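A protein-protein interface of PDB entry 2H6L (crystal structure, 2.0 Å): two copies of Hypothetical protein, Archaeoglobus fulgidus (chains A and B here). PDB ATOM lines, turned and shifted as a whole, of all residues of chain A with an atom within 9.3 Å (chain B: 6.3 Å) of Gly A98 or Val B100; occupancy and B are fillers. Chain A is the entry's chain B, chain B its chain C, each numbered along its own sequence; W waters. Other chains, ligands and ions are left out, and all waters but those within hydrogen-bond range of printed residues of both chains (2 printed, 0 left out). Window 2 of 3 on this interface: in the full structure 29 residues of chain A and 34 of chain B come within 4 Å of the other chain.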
ATOM      1  N   LEU A  73      14.527 -14.173 -31.863  1.00  0.00           N
ATOM      2  CA  LEU A  73      13.629 -15.111 -31.205  1.00  0.00           C
ATOM      3  C   LEU A  73      12.523 -15.541 -32.157  1.00  0.00           C
ATOM      4  O   LEU A  73      12.000 -16.658 -32.071  1.00  0.00           O
ATOM      5  CB  LEU A  73      13.049 -14.457 -29.956  1.00  0.00           C
ATOM      6  CG  LEU A  73      14.136 -13.927 -29.012  1.00  0.00           C
ATOM      7  CD1 LEU A  73      13.500 -13.231 -27.812  1.00  0.00           C
ATOM      8  CD2 LEU A  73      15.027 -15.095 -28.550  1.00  0.00           C
ATOM      9  N   LEU A  93      11.031 -10.474 -33.130  1.00  0.00           N
ATOM     10  CA  LEU A  93      11.109 -10.491 -31.685  1.00  0.00           C
ATOM     11  C   LEU A  93      12.591 -10.771 -31.470  1.00  0.00           C
ATOM     12  O   LEU A  93      13.115 -11.784 -31.929  1.00  0.00           O
ATOM     13  CB  LEU A  93      10.238 -11.605 -31.113  1.00  0.00           C
ATOM     14  CG  LEU A  93       8.771 -11.187 -30.939  1.00  0.00           C
ATOM     15  CD1 LEU A  93       7.836 -12.316 -31.323  1.00  0.00           C
ATOM     16  CD2 LEU A  93       8.553 -10.754 -29.502  1.00  0.00           C
ATOM     17  N   LEU A  94      13.274  -9.836 -30.823  1.00  0.00           N
ATOM     18  CA  LEU A  94      14.705  -9.973 -30.557  1.00  0.00           C
ATOM     19  C   LEU A  94      14.928  -9.887 -29.063  1.00  0.00           C
ATOM     20  O   LEU A  94      14.173  -9.226 -28.352  1.00  0.00           O
ATOM     21  CB  LEU A  94      15.491  -8.843 -31.230  1.00  0.00           C
ATOM     22  CG  LEU A  94      15.795  -8.814 -32.730  1.00  0.00           C
ATOM     23  CD1 LEU A  94      14.915  -9.773 -33.505  1.00  0.00           C
ATOM     24  CD2 LEU A  94      15.622  -7.389 -33.216  1.00  0.00           C
ATOM     25  N   GLY A  95      15.969 -10.546 -28.580  1.00  0.00           N
ATOM     26  CA  GLY A  95      16.241 -10.473 -27.161  1.00  0.00           C
ATOM     27  C   GLY A  95      16.979 -11.659 -26.597  1.00  0.00           C
ATOM     28  O   GLY A  95      17.623 -12.412 -27.323  1.00  0.00           O
ATOM     29  N   LYS A  96      16.876 -11.810 -25.283  1.00  0.00           N
ATOM     30  CA  LYS A  96      17.520 -12.899 -24.568  1.00  0.00           C
ATOM     31  C   LYS A  96      16.870 -13.030 -23.196  1.00  0.00           C
ATOM     32  O   LYS A  96      16.677 -12.033 -22.492  1.00  0.00           O
ATOM     33  CB  LYS A  96      19.019 -12.616 -24.441  1.00  0.00           C
ATOM     34  CG  LYS A  96      19.341 -11.176 -24.087  1.00  0.00           C
ATOM     35  CD  LYS A  96      20.775 -10.840 -24.445  1.00  0.00           C
ATOM     36  CE  LYS A  96      21.033  -9.345 -24.336  1.00  0.00           C
ATOM     37  NZ  LYS A  96      22.365  -8.966 -24.886  1.00  0.00           N
ATOM     38  N   ASP A  97      16.526 -14.264 -22.832  1.00  0.00           N
ATOM     39  CA  ASP A  97      15.872 -14.556 -21.559  1.00  0.00           C
ATOM     40  C   ASP A  97      14.572 -13.770 -21.446  1.00  0.00           C
ATOM     41  O   ASP A  97      13.682 -13.920 -22.274  1.00  0.00           O
ATOM     42  CB  ASP A  97      16.789 -14.208 -20.386  1.00  0.00           C
ATOM     43  CG  ASP A  97      18.055 -15.031 -20.378  1.00  0.00           C
ATOM     44  OD1 ASP A  97      17.992 -16.215 -20.781  1.00  0.00           O
ATOM     45  OD2 ASP A  97      19.107 -14.501 -19.960  1.00  0.00           O
ATOM     46  N   GLY A  98      14.474 -12.932 -20.420  1.00  0.00           N
ATOM     47  CA  GLY A  98      13.275 -12.136 -20.229  1.00  0.00           C
ATOM     48  C   GLY A  98      13.358 -10.760 -20.866  1.00  0.00           C
ATOM     49  O   GLY A  98      12.429  -9.961 -20.745  1.00  0.00           O
ATOM     50  N   GLU A  99      14.474 -10.472 -21.532  1.00  0.00           N
ATOM     51  CA  GLU A  99      14.651  -9.183 -22.198  1.00  0.00           C
ATOM     52  C   GLU A  99      14.206  -9.357 -23.638  1.00  0.00           C
ATOM     53  O   GLU A  99      14.985  -9.784 -24.490  1.00  0.00           O
ATOM     54  CB  GLU A  99      16.117  -8.753 -22.168  1.00  0.00           C
ATOM     55  CG  GLU A  99      16.361  -7.358 -22.734  1.00  0.00           C
ATOM     56  CD  GLU A  99      17.836  -7.049 -22.888  1.00  0.00           C
ATOM     57  OE1 GLU A  99      18.657  -7.862 -22.421  1.00  0.00           O
ATOM     58  OE2 GLU A  99      18.177  -5.999 -23.471  1.00  0.00           O
ATOM     59  N   VAL A 100      12.948  -9.033 -23.908  1.00  0.00           N
ATOM     60  CA  VAL A 100      12.425  -9.190 -25.252  1.00  0.00           C
ATOM     61  C   VAL A 100      11.900  -7.896 -25.854  1.00  0.00           C
ATOM     62  O   VAL A 100      11.235  -7.098 -25.191  1.00  0.00           O
ATOM     63  CB  VAL A 100      11.308 -10.252 -25.287  1.00  0.00           C
ATOM     64  CG1 VAL A 100      10.805 -10.430 -26.710  1.00  0.00           C
ATOM     65  CG2 VAL A 100      11.829 -11.576 -24.734  1.00  0.00           C
ATOM     66  N   TYR A 101      12.213  -7.702 -27.128  1.00  0.00           N
ATOM     67  CA  TYR A 101      11.781  -6.519 -27.858  1.00  0.00           C
ATOM     68  C   TYR A 101      11.068  -7.054 -29.084  1.00  0.00           C
ATOM     69  O   TYR A 101      11.326  -8.183 -29.505  1.00  0.00           O
ATOM     70  CB  TYR A 101      12.987  -5.693 -28.296  1.00  0.00           C
ATOM     71  CG  TYR A 101      13.861  -5.224 -27.162  1.00  0.00           C
ATOM     72  CD1 TYR A 101      13.465  -4.168 -26.339  1.00  0.00           C
ATOM     73  CD2 TYR A 101      15.103  -5.813 -26.927  1.00  0.00           C
ATOM     74  CE1 TYR A 101      14.297  -3.705 -25.312  1.00  0.00           C
ATOM     75  CE2 TYR A 101      15.937  -5.360 -25.902  1.00  0.00           C
ATOM     76  CZ  TYR A 101      15.532  -4.308 -25.104  1.00  0.00           C
ATOM     77  OH  TYR A 101      16.363  -3.841 -24.121  1.00  0.00           O
ATOM     78  N   LYS B  64      19.284 -20.978 -19.604  1.00  0.00           N
ATOM     79  CA  LYS B  64      18.381 -20.651 -18.518  1.00  0.00           C
ATOM     80  C   LYS B  64      17.383 -21.794 -18.328  1.00  0.00           C
ATOM     81  O   LYS B  64      16.846 -22.331 -19.294  1.00  0.00           O
ATOM     82  CB  LYS B  64      17.639 -19.358 -18.853  1.00  0.00           C
ATOM     83  CG  LYS B  64      16.753 -18.842 -17.750  1.00  0.00           C
ATOM     84  CD  LYS B  64      15.967 -17.640 -18.222  1.00  0.00           C
ATOM     85  CE  LYS B  64      15.040 -17.146 -17.134  1.00  0.00           C
ATOM     86  NZ  LYS B  64      15.803 -16.839 -15.908  1.00  0.00           N
ATOM     87  N   LEU B  73       4.636 -19.696 -27.133  1.00  0.00           N
ATOM     88  CA  LEU B  73       4.123 -18.516 -27.816  1.00  0.00           C
ATOM     89  C   LEU B  73       4.553 -18.498 -29.277  1.00  0.00           C
ATOM     90  O   LEU B  73       3.812 -18.035 -30.157  1.00  0.00           O
ATOM     91  CB  LEU B  73       4.612 -17.263 -27.099  1.00  0.00           C
ATOM     92  CG  LEU B  73       4.287 -17.282 -25.603  1.00  0.00           C
ATOM     93  CD1 LEU B  73       4.870 -16.047 -24.932  1.00  0.00           C
ATOM     94  CD2 LEU B  73       2.769 -17.341 -25.409  1.00  0.00           C
ATOM     95  N   LEU B  93       9.744 -18.762 -27.963  1.00  0.00           N
ATOM     96  CA  LEU B  93       9.252 -17.716 -27.097  1.00  0.00           C
ATOM     97  C   LEU B  93       8.244 -18.488 -26.246  1.00  0.00           C
ATOM     98  O   LEU B  93       7.302 -19.092 -26.765  1.00  0.00           O
ATOM     99  CB  LEU B  93       8.590 -16.608 -27.921  1.00  0.00           C
ATOM    100  CG  LEU B  93       9.616 -15.635 -28.531  1.00  0.00           C
ATOM    101  CD1 LEU B  93       9.214 -15.203 -29.918  1.00  0.00           C
ATOM    102  CD2 LEU B  93       9.767 -14.442 -27.604  1.00  0.00           C
ATOM    103  N   LEU B  94       8.493 -18.525 -24.946  1.00  0.00           N
ATOM    104  CA  LEU B  94       7.626 -19.234 -24.011  1.00  0.00           C
ATOM    105  C   LEU B  94       7.189 -18.260 -22.946  1.00  0.00           C
ATOM    106  O   LEU B  94       7.917 -17.329 -22.609  1.00  0.00           O
ATOM    107  CB  LEU B  94       8.374 -20.379 -23.323  1.00  0.00           C
ATOM    108  CG  LEU B  94       8.795 -21.659 -24.046  1.00  0.00           C
ATOM    109  CD1 LEU B  94       8.530 -21.577 -25.537  1.00  0.00           C
ATOM    110  CD2 LEU B  94      10.265 -21.905 -23.754  1.00  0.00           C
ATOM    111  N   GLY B  95       6.001 -18.480 -22.405  1.00  0.00           N
ATOM    112  CA  GLY B  95       5.522 -17.599 -21.361  1.00  0.00           C
ATOM    113  C   GLY B  95       4.019 -17.553 -21.262  1.00  0.00           C
ATOM    114  O   GLY B  95       3.326 -18.426 -21.775  1.00  0.00           O
ATOM    115  N   LYS B  96       3.526 -16.520 -20.590  1.00  0.00           N
ATOM    116  CA  LYS B  96       2.101 -16.314 -20.400  1.00  0.00           C
ATOM    117  C   LYS B  96       1.902 -14.856 -20.021  1.00  0.00           C
ATOM    118  O   LYS B  96       2.640 -14.316 -19.192  1.00  0.00           O
ATOM    119  CB  LYS B  96       1.582 -17.234 -19.295  1.00  0.00           C
ATOM    120  CG  LYS B  96       2.499 -17.307 -18.086  1.00  0.00           C
ATOM    121  CD  LYS B  96       2.231 -18.563 -17.274  1.00  0.00           C
ATOM    122  CE  LYS B  96       3.306 -18.769 -16.216  1.00  0.00           C
ATOM    123  NZ  LYS B  96       3.213 -20.108 -15.568  1.00  0.00           N
ATOM    124  N   ASP B  97       0.910 -14.223 -20.642  1.00  0.00           N
ATOM    125  CA  ASP B  97       0.618 -12.817 -20.401  1.00  0.00           C
ATOM    126  C   ASP B  97       1.866 -11.991 -20.677  1.00  0.00           C
ATOM    127  O   ASP B  97       2.476 -12.121 -21.735  1.00  0.00           O
ATOM    128  CB  ASP B  97       0.156 -12.604 -18.962  1.00  0.00           C
ATOM    129  CG  ASP B  97      -1.176 -13.257 -18.686  1.00  0.00           C
ATOM    130  OD1 ASP B  97      -1.884 -13.586 -19.667  1.00  0.00           O
ATOM    131  OD2 ASP B  97      -1.522 -13.429 -17.497  1.00  0.00           O
ATOM    132  N   GLY B  98       2.246 -11.151 -19.720  1.00  0.00           N
ATOM    133  CA  GLY B  98       3.423 -10.323 -19.891  1.00  0.00           C
ATOM    134  C   GLY B  98       4.717 -11.016 -19.503  1.00  0.00           C
ATOM    135  O   GLY B  98       5.786 -10.411 -19.579  1.00  0.00           O
ATOM    136  N   GLU B  99       4.628 -12.273 -19.069  1.00  0.00           N
ATOM    137  CA  GLU B  99       5.821 -13.031 -18.691  1.00  0.00           C
ATOM    138  C   GLU B  99       6.311 -13.770 -19.928  1.00  0.00           C
ATOM    139  O   GLU B  99       5.762 -14.807 -20.302  1.00  0.00           O
ATOM    140  CB  GLU B  99       5.502 -14.032 -17.575  1.00  0.00           C
ATOM    141  CG  GLU B  99       6.732 -14.759 -17.025  1.00  0.00           C
ATOM    142  CD  GLU B  99       6.431 -15.592 -15.786  1.00  0.00           C
ATOM    143  OE1 GLU B  99       5.752 -15.072 -14.879  1.00  0.00           O
ATOM    144  OE2 GLU B  99       6.885 -16.755 -15.705  1.00  0.00           O
ATOM    145  N   VAL B 100       7.339 -13.228 -20.572  1.00  0.00           N
ATOM    146  CA  VAL B 100       7.860 -13.854 -21.779  1.00  0.00           C
ATOM    147  C   VAL B 100       9.360 -14.096 -21.737  1.00  0.00           C
ATOM    148  O   VAL B 100      10.132 -13.231 -21.324  1.00  0.00           O
ATOM    149  CB  VAL B 100       7.528 -13.013 -23.029  1.00  0.00           C
ATOM    150  CG1 VAL B 100       8.101 -13.679 -24.278  1.00  0.00           C
ATOM    151  CG2 VAL B 100       6.017 -12.849 -23.158  1.00  0.00           C
ATOM    152  N   TYR B 101       9.752 -15.290 -22.173  1.00  0.00           N
ATOM    153  CA  TYR B 101      11.154 -15.702 -22.218  1.00  0.00           C
ATOM    154  C   TYR B 101      11.423 -16.125 -23.650  1.00  0.00           C
ATOM    155  O   TYR B 101      10.528 -16.637 -24.324  1.00  0.00           O
ATOM    156  CB  TYR B 101      11.393 -16.904 -21.306  1.00  0.00           C
ATOM    157  CG  TYR B 101      10.985 -16.688 -19.874  1.00  0.00           C
ATOM    158  CD1 TYR B 101      11.735 -15.873 -19.026  1.00  0.00           C
ATOM    159  CD2 TYR B 101       9.852 -17.312 -19.356  1.00  0.00           C
ATOM    160  CE1 TYR B 101      11.363 -15.690 -17.688  1.00  0.00           C
ATOM    161  CE2 TYR B 101       9.473 -17.133 -18.028  1.00  0.00           C
ATOM    162  CZ  TYR B 101      10.228 -16.330 -17.200  1.00  0.00           C
ATOM    163  OH  TYR B 101       9.860 -16.187 -15.891  1.00  0.00           O
ATOM    164  N   GLY B 102      12.643 -15.918 -24.124  1.00  0.00           N
ATOM    165  CA  GLY B 102      12.945 -16.317 -25.486  1.00  0.00           C
ATOM    166  C   GLY B 102      14.392 -16.711 -25.688  1.00  0.00           C
ATOM    167  O   GLY B 102      15.260 -16.308 -24.918  1.00  0.00           O
HETATM  168  O   HOH W   1      19.704 -18.080 -21.315  1.00  0.00           O
HETATM  169  O   HOH W   2      17.983 -16.509 -23.594  1.00  0.00           O
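The backbone carbonyl oxygen (O) of Asp A97 is in hydrogen-bond range of the backbone NH (N) of Gly B102 (2.9 Å).
The backbone NH (N) of Leu A73 is in hydrogen-bond range of the backbone carbonyl oxygen (O) of Leu A93 (2.8 Å).
The backbone carbonyl oxygen (O) of Leu B93 sits at hydrogen-bond distance from the backbone NH (N) of Leu B73, at 2.8 Å.
The backbone carbonyl oxygen (O) of Leu B94 is in hydrogen-bond range of the backbone NH (N) of Tyr B101.
OE2 of Glu B99 lies within hydrogen-bond range of OH of Tyr B101.
Leu A73 touches Leu B93.
Gly B102 touches Leu A73 (C to CD2, 3.3 Å).
Leu B93 touches Leu A93 (CD1 to CD1, 3.5 Å).
Asp A97 touches Lys B64 (OD1 to CD, 3.6 Å).
O of Asp A97 touches O of Val B100 (3.7 Å).
Tyr B101 touches Asp A97.
O of Val B100 touches CA of Gly A98 (3.5 Å).
Printed residues of chain B within 4 Å of Leu A93: Leu B93.
Of the printed residues of chain B, Asp A97 touches Lys B64, Val B100, Tyr B101 and Gly B102.
Gly A98 touches one residue of chain B.
Printed residues of chain A within 4 Å of Leu B93: Leu A73 and Leu A93.
Val B100 touches just these residues of chain A: Asp A97 (3.7 Å) and Gly A98 (3.5 Å).
Printed residues of chain A within 4 Å of Tyr B101: Asp A97 (3.1 Å).
Printed residues of chain A within 4 Å of Gly B102: Leu A73 and Asp A97.
The nearest residue of chain B that does not touch Gly A98 is Tyr B101 (4.2 Å).
The nearest residue of chain A that does not touch Val B100 is Val A100 (4.2 Å).
Of the 10 printed residues of chain A, 4 touch a printed residue of chain B.
Of the 12 printed residues of chain B, 5 touch a printed residue of chain A.
Hydrophobic or aromatic side chains of chain B within 4 Å of the printed part of chain A: Leu B93 and Tyr B101.
Along chain B the printed residues that touch a printed residue of chain A span positions 64 to 102.
Among the printed residues, 8 pairs touch across the chains.
Among the printed residues, no Asp or Glu carboxylate lies within 4 Å of a Lys or Arg side-chain nitrogen of the other chain.
Leu A73 touches Leu B93, but with the chains exchanged Leu A93 does not touch Leu B73 (7.1 Å).
Leu B93 touches its own counterpart, Leu A93.
Asp A97 touches Val B100, but with the chains exchanged Val A100 does not touch Asp B97 (9.7 Å).
Asp A97 touches Tyr B101, but with the chains exchanged Tyr A101 does not touch Asp B97 (12.0 Å).
Positions printed for both chains: 73, 93, 94, 95, 96, 97, 98, 99, 100 and 101.
Of the 8 pairs that touch across the chains among the printed residues, 1 has its exchanged pair printed and touching as well.
Water W1 bridges OD1 of Asp A97 (2.6 Å) and N of Lys B64 (3.4 Å).
Water W2 lies within hydrogen-bond range of the backbone NH of Asp A97 and the backbone carbonyl oxygen of Gly B102.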
